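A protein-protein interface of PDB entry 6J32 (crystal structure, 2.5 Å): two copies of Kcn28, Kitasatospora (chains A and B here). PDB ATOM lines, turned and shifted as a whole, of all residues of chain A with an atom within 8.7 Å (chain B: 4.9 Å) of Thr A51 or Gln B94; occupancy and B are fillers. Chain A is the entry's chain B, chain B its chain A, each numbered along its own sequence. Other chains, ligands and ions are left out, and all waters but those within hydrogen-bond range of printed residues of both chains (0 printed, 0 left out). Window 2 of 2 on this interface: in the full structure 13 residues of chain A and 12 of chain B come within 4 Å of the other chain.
No position is printed for both chains.
Of the 8 pairs that touch across the chains among the printed residues, none has its exchanged pair printed and touching as well.
Val A32 touches none of the printed residues of chain B.
Asn A42 touches none of the printed residues of chain B.
Of the printed residues of chain B, Ala A48 touches Gly B90 and Gln B94.
Printed residues of chain B within 4 Å of Glu A52: Pro B93 (3.6 Å).
Of the printed residues of chain A, Gly B90 touches Ala A48 (3.6 Å).
Printed residues of chain A within 4 Å of Pro B93: Thr A51 and Glu A52.
Gln B94 touches just these residues of chain A: Ala A47, Ala A48 and Thr A51.
The nearest residue of chain A that does not touch Gln B94 is Pro A44 (5.3 Å).
The nearest printed residue of chain B that does not touch Glu A52 is Gln B94 (5.8 Å).
CB of Ala A47 touches OG1 of Thr B61, at 3.7 Å.
Gln B94 touches Ala A47 (OE1 to CB, 3.5 Å).
Ala A48 touches Gly B90.
Ala A48 touches Gln B94 (CB to NE2, 3.98 Å).
Pro B93 touches Thr A51.
OG1 of Thr A51 touches N of Gln B94, 3.6 Å away.
CB of Pro B93 touches N of Glu A52, at 3.6 Å.
OE1 of Gln B94 lies within hydrogen-bond range of N of Thr B61 (2.7 Å).
O of Gly B90 sits at hydrogen-bond distance from NE2 of Gln B94.
NH2 of Arg A29 is in salt-bridge range of OE1 of Glu A52, at 2.6 Å.
The backbone carbonyl oxygen (O) of Ala A47 sits at hydrogen-bond distance from the side-chain hydroxyl (OG1) of Thr A51, 2.8 Å away.
The side-chain hydroxyl (OG1) of Thr A51 sits at hydrogen-bond distance from the backbone carbonyl oxygen (O) of Ala A48 (3.0 Å).
The backbone carbonyl oxygen (O) of Pro A44 lies within hydrogen-bond range of the side-chain hydroxyl (OG1) of Thr B61, at 2.5 Å.
Of the 11 printed residues of chain B, 4 touch a printed residue of chain A.
Of the 23 printed residues of chain A, 5 touch a printed residue of chain B.
Hydrophobic or aromatic side chains of chain A within 4 Å of the printed part of chain B: Ala A47 and Ala A48.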
ATOM      1  N   LEU A  21       6.732  24.394 -22.379  1.00  0.00           N
ATOM      2  CA  LEU A  21       8.065  24.922 -22.599  1.00  0.00           C
ATOM      3  C   LEU A  21       8.156  26.412 -22.311  1.00  0.00           C
ATOM      4  O   LEU A  21       8.993  26.836 -21.505  1.00  0.00           O
ATOM      5  CB  LEU A  21       8.458  24.648 -24.052  1.00  0.00           C
ATOM      6  CG  LEU A  21       9.812  25.170 -24.486  1.00  0.00           C
ATOM      7  CD1 LEU A  21      10.906  24.272 -23.936  1.00  0.00           C
ATOM      8  CD2 LEU A  21       9.819  25.239 -25.980  1.00  0.00           C
ATOM      9  N   LEU A  25      10.637  29.334 -19.385  1.00  0.00           N
ATOM     10  CA  LEU A  25      11.880  29.757 -20.026  1.00  0.00           C
ATOM     11  C   LEU A  25      12.592  30.830 -19.207  1.00  0.00           C
ATOM     12  O   LEU A  25      13.785  30.707 -18.906  1.00  0.00           O
ATOM     13  CB  LEU A  25      11.590  30.262 -21.440  1.00  0.00           C
ATOM     14  CG  LEU A  25      11.817  29.313 -22.625  1.00  0.00           C
ATOM     15  CD1 LEU A  25      11.942  27.855 -22.201  1.00  0.00           C
ATOM     16  CD2 LEU A  25      10.711  29.475 -23.661  1.00  0.00           C
ATOM     17  N   ILE A  28      14.210  29.543 -15.987  1.00  0.00           N
ATOM     18  CA  ILE A  28      15.490  28.867 -16.164  1.00  0.00           C
ATOM     19  C   ILE A  28      16.586  29.886 -16.443  1.00  0.00           C
ATOM     20  O   ILE A  28      17.698  29.782 -15.911  1.00  0.00           O
ATOM     21  CB  ILE A  28      15.395  27.814 -17.280  1.00  0.00           C
ATOM     22  CG1 ILE A  28      14.254  26.833 -17.012  1.00  0.00           C
ATOM     23  CG2 ILE A  28      16.669  27.025 -17.338  1.00  0.00           C
ATOM     24  CD1 ILE A  28      14.433  26.034 -15.750  1.00  0.00           C
ATOM     25  N   ARG A  29      16.276  30.908 -17.249  1.00  0.00           N
ATOM     26  CA  ARG A  29      17.239  31.969 -17.532  1.00  0.00           C
ATOM     27  C   ARG A  29      17.678  32.678 -16.256  1.00  0.00           C
ATOM     28  O   ARG A  29      18.857  33.022 -16.102  1.00  0.00           O
ATOM     29  CB  ARG A  29      16.636  32.970 -18.517  1.00  0.00           C
ATOM     30  CG  ARG A  29      17.567  34.110 -18.905  1.00  0.00           C
ATOM     31  CD  ARG A  29      16.857  35.167 -19.761  1.00  0.00           C
ATOM     32  NE  ARG A  29      15.876  34.575 -20.670  1.00  0.00           N
ATOM     33  CZ  ARG A  29      16.169  34.074 -21.868  1.00  0.00           C
ATOM     34  NH1 ARG A  29      17.421  34.083 -22.307  1.00  0.00           N
ATOM     35  NH2 ARG A  29      15.210  33.551 -22.625  1.00  0.00           N
ATOM     36  N   VAL A  32      20.089  30.518 -14.396  1.00  0.00           N
ATOM     37  CA  VAL A  32      21.406  30.595 -15.016  1.00  0.00           C
ATOM     38  C   VAL A  32      22.076  31.916 -14.661  1.00  0.00           C
ATOM     39  O   VAL A  32      23.265  31.953 -14.319  1.00  0.00           O
ATOM     40  CB  VAL A  32      21.294  30.398 -16.540  1.00  0.00           C
ATOM     41  CG1 VAL A  32      22.652  30.558 -17.204  1.00  0.00           C
ATOM     42  CG2 VAL A  32      20.724  29.026 -16.854  1.00  0.00           C
ATOM     43  N   TYR A  40      18.885  21.093 -18.878  1.00  0.00           N
ATOM     44  CA  TYR A  40      17.490  21.073 -19.298  1.00  0.00           C
ATOM     45  C   TYR A  40      17.300  19.873 -20.214  1.00  0.00           C
ATOM     46  O   TYR A  40      17.789  19.871 -21.347  1.00  0.00           O
ATOM     47  CB  TYR A  40      17.125  22.386 -19.992  1.00  0.00           C
ATOM     48  CG  TYR A  40      15.643  22.636 -20.189  1.00  0.00           C
ATOM     49  CD1 TYR A  40      14.737  21.586 -20.309  1.00  0.00           C
ATOM     50  CD2 TYR A  40      15.155  23.930 -20.265  1.00  0.00           C
ATOM     51  CE1 TYR A  40      13.396  21.821 -20.497  1.00  0.00           C
ATOM     52  CE2 TYR A  40      13.812  24.175 -20.450  1.00  0.00           C
ATOM     53  CZ  TYR A  40      12.938  23.118 -20.565  1.00  0.00           C
ATOM     54  OH  TYR A  40      11.601  23.364 -20.750  1.00  0.00           O
ATOM     55  N   ASN A  42      15.085  17.714 -22.575  1.00  0.00           N
ATOM     56  CA  ASN A  42      13.903  17.801 -23.418  1.00  0.00           C
ATOM     57  C   ASN A  42      14.222  17.135 -24.748  1.00  0.00           C
ATOM     58  O   ASN A  42      15.354  16.715 -25.000  1.00  0.00           O
ATOM     59  CB  ASN A  42      13.471  19.258 -23.621  1.00  0.00           C
ATOM     60  CG  ASN A  42      11.970  19.408 -23.753  1.00  0.00           C
ATOM     61  OD1 ASN A  42      11.289  18.535 -24.295  1.00  0.00           O
ATOM     62  ND2 ASN A  42      11.444  20.530 -23.273  1.00  0.00           N
ATOM     63  N   ASP A  43      13.205  17.038 -25.594  1.00  0.00           N
ATOM     64  CA  ASP A  43      13.394  16.474 -26.919  1.00  0.00           C
ATOM     65  C   ASP A  43      14.169  17.453 -27.800  1.00  0.00           C
ATOM     66  O   ASP A  43      13.971  18.668 -27.701  1.00  0.00           O
ATOM     67  CB  ASP A  43      12.033  16.148 -27.527  1.00  0.00           C
ATOM     68  CG  ASP A  43      12.136  15.408 -28.840  1.00  0.00           C
ATOM     69  OD1 ASP A  43      12.404  16.062 -29.869  1.00  0.00           O
ATOM     70  OD2 ASP A  43      11.963  14.167 -28.832  1.00  0.00           O
ATOM     71  N   PRO A  44      15.062  16.962 -28.669  1.00  0.00           N
ATOM     72  CA  PRO A  44      15.851  17.880 -29.515  1.00  0.00           C
ATOM     73  C   PRO A  44      15.022  18.697 -30.484  1.00  0.00           C
ATOM     74  O   PRO A  44      15.536  19.694 -31.013  1.00  0.00           O
ATOM     75  CB  PRO A  44      16.803  16.939 -30.267  1.00  0.00           C
ATOM     76  CG  PRO A  44      16.135  15.608 -30.214  1.00  0.00           C
ATOM     77  CD  PRO A  44      15.463  15.560 -28.876  1.00  0.00           C
ATOM     78  N   SER A  45      13.759  18.337 -30.718  1.00  0.00           N
ATOM     79  CA  SER A  45      12.922  19.128 -31.611  1.00  0.00           C
ATOM     80  C   SER A  45      12.679  20.519 -31.064  1.00  0.00           C
ATOM     81  O   SER A  45      12.319  21.424 -31.822  1.00  0.00           O
ATOM     82  CB  SER A  45      11.574  18.443 -31.833  1.00  0.00           C
ATOM     83  OG  SER A  45      10.842  18.368 -30.621  1.00  0.00           O
ATOM     84  N   VAL A  46      12.886  20.714 -29.771  1.00  0.00           N
ATOM     85  CA  VAL A  46      12.670  21.997 -29.129  1.00  0.00           C
ATOM     86  C   VAL A  46      13.990  22.578 -28.590  1.00  0.00           C
ATOM     87  O   VAL A  46      13.997  23.480 -27.754  1.00  0.00           O
ATOM     88  CB  VAL A  46      11.564  21.829 -28.063  1.00  0.00           C
ATOM     89  CG1 VAL A  46      12.083  21.685 -26.617  1.00  0.00           C
ATOM     90  CG2 VAL A  46      10.485  22.857 -28.234  1.00  0.00           C
ATOM     91  N   ALA A  47      15.115  22.141 -29.171  1.00  0.00           N
ATOM     92  CA  ALA A  47      16.443  22.540 -28.705  1.00  0.00           C
ATOM     93  C   ALA A  47      16.706  24.037 -28.832  1.00  0.00           C
ATOM     94  O   ALA A  47      17.503  24.588 -28.060  1.00  0.00           O
ATOM     95  CB  ALA A  47      17.519  21.763 -29.459  1.00  0.00           C
ATOM     96  N   ALA A  48      16.082  24.713 -29.798  1.00  0.00           N
ATOM     97  CA  ALA A  48      16.310  26.151 -29.928  1.00  0.00           C
ATOM     98  C   ALA A  48      15.883  26.890 -28.665  1.00  0.00           C
ATOM     99  O   ALA A  48      16.660  27.659 -28.088  1.00  0.00           O
ATOM    100  CB  ALA A  48      15.575  26.700 -31.151  1.00  0.00           C
ATOM    101  N   ALA A  49      14.648  26.655 -28.214  1.00  0.00           N
ATOM    102  CA  ALA A  49      14.145  27.350 -27.031  1.00  0.00           C
ATOM    103  C   ALA A  49      14.932  26.970 -25.782  1.00  0.00           C
ATOM    104  O   ALA A  49      15.169  27.812 -24.909  1.00  0.00           O
ATOM    105  CB  ALA A  49      12.660  27.049 -26.841  1.00  0.00           C
ATOM    106  N   VAL A  50      15.336  25.704 -25.672  1.00  0.00           N
ATOM    107  CA  VAL A  50      16.086  25.268 -24.496  1.00  0.00           C
ATOM    108  C   VAL A  50      17.441  25.966 -24.437  1.00  0.00           C
ATOM    109  O   VAL A  50      17.839  26.497 -23.393  1.00  0.00           O
ATOM    110  CB  VAL A  50      16.231  23.734 -24.494  1.00  0.00           C
ATOM    111  CG1 VAL A  50      17.139  23.287 -23.365  1.00  0.00           C
ATOM    112  CG2 VAL A  50      14.863  23.070 -24.378  1.00  0.00           C
ATOM    113  N   THR A  51      18.166  25.988 -25.561  1.00  0.00           N
ATOM    114  CA  THR A  51      19.506  26.571 -25.561  1.00  0.00           C
ATOM    115  C   THR A  51      19.475  28.085 -25.391  1.00  0.00           C
ATOM    116  O   THR A  51      20.379  28.648 -24.764  1.00  0.00           O
ATOM    117  CB  THR A  51      20.247  26.209 -26.852  1.00  0.00           C
ATOM    118  OG1 THR A  51      19.461  26.601 -27.983  1.00  0.00           O
ATOM    119  CG2 THR A  51      20.513  24.705 -26.917  1.00  0.00           C
ATOM    120  N   GLU A  52      18.458  28.762 -25.941  1.00  0.00           N
ATOM    121  CA  GLU A  52      18.387  30.217 -25.815  1.00  0.00           C
ATOM    122  C   GLU A  52      18.321  30.631 -24.352  1.00  0.00           C
ATOM    123  O   GLU A  52      18.773  31.721 -23.984  1.00  0.00           O
ATOM    124  CB  GLU A  52      17.178  30.755 -26.584  1.00  0.00           C
ATOM    125  CG  GLU A  52      17.285  32.221 -26.989  1.00  0.00           C
ATOM    126  CD  GLU A  52      16.761  33.187 -25.934  1.00  0.00           C
ATOM    127  OE1 GLU A  52      16.237  32.728 -24.898  1.00  0.00           O
ATOM    128  OE2 GLU A  52      16.885  34.415 -26.138  1.00  0.00           O
ATOM    129  N   THR A  53      17.776  29.757 -23.511  1.00  0.00           N
ATOM    130  CA  THR A  53      17.723  29.992 -22.077  1.00  0.00           C
ATOM    131  C   THR A  53      19.117  30.120 -21.472  1.00  0.00           C
ATOM    132  O   THR A  53      19.301  30.831 -20.475  1.00  0.00           O
ATOM    133  CB  THR A  53      16.951  28.838 -21.434  1.00  0.00           C
ATOM    134  OG1 THR A  53      15.662  29.285 -20.998  1.00  0.00           O
ATOM    135  CG2 THR A  53      17.714  28.253 -20.286  1.00  0.00           C
ATOM    136  N   GLY A  54      20.108  29.467 -22.073  1.00  0.00           N
ATOM    137  CA  GLY A  54      21.442  29.393 -21.519  1.00  0.00           C
ATOM    138  C   GLY A  54      21.737  28.126 -20.750  1.00  0.00           C
ATOM    139  O   GLY A  54      22.819  28.017 -20.164  1.00  0.00           O
ATOM    140  N   ALA A  55      20.822  27.166 -20.745  1.00  0.00           N
ATOM    141  CA  ALA A  55      21.008  25.919 -20.026  1.00  0.00           C
ATOM    142  C   ALA A  55      21.598  24.845 -20.934  1.00  0.00           C
ATOM    143  O   ALA A  55      21.492  24.900 -22.162  1.00  0.00           O
ATOM    144  CB  ALA A  55      19.681  25.434 -19.443  1.00  0.00           C
ATOM    145  N   GLU A  56      22.223  23.858 -20.301  1.00  0.00           N
ATOM    146  CA  GLU A  56      22.776  22.709 -21.007  1.00  0.00           C
ATOM    147  C   GLU A  56      21.638  21.803 -21.462  1.00  0.00           C
ATOM    148  O   GLU A  56      20.918  21.241 -20.629  1.00  0.00           O
ATOM    149  CB  GLU A  56      23.724  21.952 -20.076  1.00  0.00           C
ATOM    150  CG  GLU A  56      24.808  21.116 -20.739  1.00  0.00           C
ATOM    151  CD  GLU A  56      25.669  20.383 -19.713  1.00  0.00           C
ATOM    152  OE1 GLU A  56      26.104  21.025 -18.729  1.00  0.00           O
ATOM    153  OE2 GLU A  56      25.898  19.164 -19.880  1.00  0.00           O
ATOM    154  N   LEU A  57      21.474  21.648 -22.774  1.00  0.00           N
ATOM    155  CA  LEU A  57      20.435  20.759 -23.280  1.00  0.00           C
ATOM    156  C   LEU A  57      20.835  19.306 -23.069  1.00  0.00           C
ATOM    157  O   LEU A  57      21.923  18.887 -23.473  1.00  0.00           O
ATOM    158  CB  LEU A  57      20.171  21.009 -24.762  1.00  0.00           C
ATOM    159  CG  LEU A  57      19.323  19.902 -25.404  1.00  0.00           C
ATOM    160  CD1 LEU A  57      17.894  19.916 -24.863  1.00  0.00           C
ATOM    161  CD2 LEU A  57      19.326  19.993 -26.926  1.00  0.00           C
ATOM    162  N   VAL A  58      19.948  18.536 -22.450  1.00  0.00           N
ATOM    163  CA  VAL A  58      20.163  17.103 -22.258  1.00  0.00           C
ATOM    164  C   VAL A  58      19.124  16.372 -23.099  1.00  0.00           C
ATOM    165  O   VAL A  58      17.976  16.209 -22.667  1.00  0.00           O
ATOM    166  CB  VAL A  58      20.067  16.712 -20.775  1.00  0.00           C
ATOM    167  CG1 VAL A  58      20.211  15.208 -20.610  1.00  0.00           C
ATOM    168  CG2 VAL A  58      21.126  17.443 -19.966  1.00  0.00           C
ATOM    169  N   TYR B  60      22.690  20.533 -34.431  1.00  0.00           N
ATOM    170  CA  TYR B  60      21.697  21.518 -34.037  1.00  0.00           C
ATOM    171  C   TYR B  60      20.417  21.178 -34.780  1.00  0.00           C
ATOM    172  O   TYR B  60      20.456  20.603 -35.868  1.00  0.00           O
ATOM    173  CB  TYR B  60      22.154  22.966 -34.328  1.00  0.00           C
ATOM    174  CG  TYR B  60      22.050  23.411 -35.777  1.00  0.00           C
ATOM    175  CD1 TYR B  60      20.845  23.864 -36.308  1.00  0.00           C
ATOM    176  CD2 TYR B  60      23.165  23.391 -36.612  1.00  0.00           C
ATOM    177  CE1 TYR B  60      20.750  24.271 -37.628  1.00  0.00           C
ATOM    178  CE2 TYR B  60      23.080  23.799 -37.932  1.00  0.00           C
ATOM    179  CZ  TYR B  60      21.873  24.237 -38.435  1.00  0.00           C
ATOM    180  OH  TYR B  60      21.780  24.644 -39.747  1.00  0.00           O
ATOM    181  N   THR B  61      19.283  21.545 -34.194  1.00  0.00           N
ATOM    182  CA  THR B  61      17.989  21.222 -34.777  1.00  0.00           C
ATOM    183  C   THR B  61      17.620  22.290 -35.795  1.00  0.00           C
ATOM    184  O   THR B  61      17.545  23.478 -35.461  1.00  0.00           O
ATOM    185  CB  THR B  61      16.905  21.110 -33.707  1.00  0.00           C
ATOM    186  OG1 THR B  61      17.242  20.066 -32.780  1.00  0.00           O
ATOM    187  CG2 THR B  61      15.565  20.792 -34.361  1.00  0.00           C
ATOM    188  N   GLY B  90      16.218  30.219 -34.568  1.00  0.00           N
ATOM    189  CA  GLY B  90      16.517  29.004 -33.833  1.00  0.00           C
ATOM    190  C   GLY B  90      17.966  28.564 -33.912  1.00  0.00           C
ATOM    191  O   GLY B  90      18.470  27.930 -32.982  1.00  0.00           O
ATOM    192  N   MET B  91      18.652  28.877 -35.018  1.00  0.00           N
ATOM    193  CA  MET B  91      20.016  28.378 -35.197  1.00  0.00           C
ATOM    194  C   MET B  91      20.999  29.051 -34.248  1.00  0.00           C
ATOM    195  O   MET B  91      21.871  28.386 -33.676  1.00  0.00           O
ATOM    196  CB  MET B  91      20.471  28.571 -36.641  1.00  0.00           C
ATOM    197  CG  MET B  91      21.815  27.931 -36.930  1.00  0.00           C
ATOM    198  SD  MET B  91      22.445  28.320 -38.564  1.00  0.00           S
ATOM    199  CE  MET B  91      21.052  27.829 -39.582  1.00  0.00           C
ATOM    200  N   LEU B  92      20.873  30.362 -34.064  1.00  0.00           N
ATOM    201  CA  LEU B  92      21.881  31.105 -33.310  1.00  0.00           C
ATOM    202  C   LEU B  92      22.073  30.596 -31.887  1.00  0.00           C
ATOM    203  O   LEU B  92      23.230  30.384 -31.489  1.00  0.00           O
ATOM    204  CB  LEU B  92      21.541  32.599 -33.333  1.00  0.00           C
ATOM    205  CG  LEU B  92      22.389  33.521 -32.459  1.00  0.00           C
ATOM    206  CD1 LEU B  92      23.834  33.463 -32.886  1.00  0.00           C
ATOM    207  CD2 LEU B  92      21.868  34.948 -32.577  1.00  0.00           C
ATOM    208  N   PRO B  93      21.028  30.376 -31.076  1.00  0.00           N
ATOM    209  CA  PRO B  93      21.280  29.885 -29.709  1.00  0.00           C
ATOM    210  C   PRO B  93      21.940  28.522 -29.669  1.00  0.00           C
ATOM    211  O   PRO B  93      22.737  28.257 -28.761  1.00  0.00           O
ATOM    212  CB  PRO B  93      19.879  29.833 -29.081  1.00  0.00           C
ATOM    213  CG  PRO B  93      18.993  30.623 -29.980  1.00  0.00           C
ATOM    214  CD  PRO B  93      19.585  30.514 -31.343  1.00  0.00           C
ATOM    215  N   GLN B  94      21.621  27.639 -30.617  1.00  0.00           N
ATOM    216  CA  GLN B  94      22.248  26.321 -30.632  1.00  0.00           C
ATOM    217  C   GLN B  94      23.732  26.414 -30.969  1.00  0.00           C
ATOM    218  O   GLN B  94      24.557  25.721 -30.361  1.00  0.00           O
ATOM    219  CB  GLN B  94      21.511  25.409 -31.612  1.00  0.00           C
ATOM    220  CG  GLN B  94      20.015  25.342 -31.347  1.00  0.00           C
ATOM    221  CD  GLN B  94      19.309  24.292 -32.174  1.00  0.00           C
ATOM    222  OE1 GLN B  94      19.528  23.092 -31.998  1.00  0.00           O
ATOM    223  NE2 GLN B  94      18.447  24.739 -33.082  1.00  0.00           N
ATOM    224  N   LEU B  95      24.097  27.282 -31.919  1.00  0.00           N
ATOM    225  CA  LEU B  95      25.514  27.488 -32.209  1.00  0.00           C
ATOM    226  C   LEU B  95      26.221  28.124 -31.021  1.00  0.00           C
ATOM    227  O   LEU B  95      27.367  27.771 -30.711  1.00  0.00           O
ATOM    228  CB  LEU B  95      25.685  28.348 -33.463  1.00  0.00           C
ATOM    229  CG  LEU B  95      25.109  27.781 -34.761  1.00  0.00           C
ATOM    230  CD1 LEU B  95      25.263  28.774 -35.903  1.00  0.00           C
ATOM    231  CD2 LEU B  95      25.758  26.446 -35.100  1.00  0.00           C
ATOM    232  N   ARG B  96      25.549  29.056 -30.339  1.00  0.00           N
ATOM    233  CA  ARG B  96      26.148  29.699 -29.175  1.00  0.00           C
ATOM    234  C   ARG B  96      26.453  28.678 -28.088  1.00  0.00           C
ATOM    235  O   ARG B  96      27.576  28.614 -27.575  1.00  0.00           O
ATOM    236  CB  ARG B  96      25.209  30.779 -28.631  1.00  0.00           C
ATOM    237  CG  ARG B  96      25.844  31.685 -27.581  1.00  0.00           C
ATOM    238  CD  ARG B  96      24.835  32.662 -26.996  1.00  0.00           C
ATOM    239  NE  ARG B  96      24.266  33.559 -27.999  1.00  0.00           N
ATOM    240  CZ  ARG B  96      24.866  34.653 -28.460  1.00  0.00           C
ATOM    241  NH1 ARG B  96      26.072  34.990 -28.018  1.00  0.00           N
ATOM    242  NH2 ARG B  96      24.264  35.408 -29.369  1.00  0.00           N
ATOM    243  N   ALA B  97      25.470  27.838 -27.754  1.00  0.00           N
ATOM    244  CA  ALA B  97      25.673  26.834 -26.714  1.00  0.00           C
ATOM    245  C   ALA B  97      26.756  25.836 -27.105  1.00  0.00           C
ATOM    246  O   ALA B  97      27.563  25.427 -26.263  1.00  0.00           O
ATOM    247  CB  ALA B  97      24.358  26.112 -26.420  1.00  0.00           C
ATOM    248  N   ALA B  98      26.799  25.443 -28.377  1.00  0.00           N
ATOM    249  CA  ALA B  98      27.761  24.429 -28.792  1.00  0.00           C
ATOM    250  C   ALA B  98      29.191  24.959 -28.750  1.00  0.00           C
ATOM    251  O   ALA B  98      30.112  24.237 -28.355  1.00  0.00           O
ATOM    252  CB  ALA B  98      27.420  23.924 -30.192  1.00  0.00           C
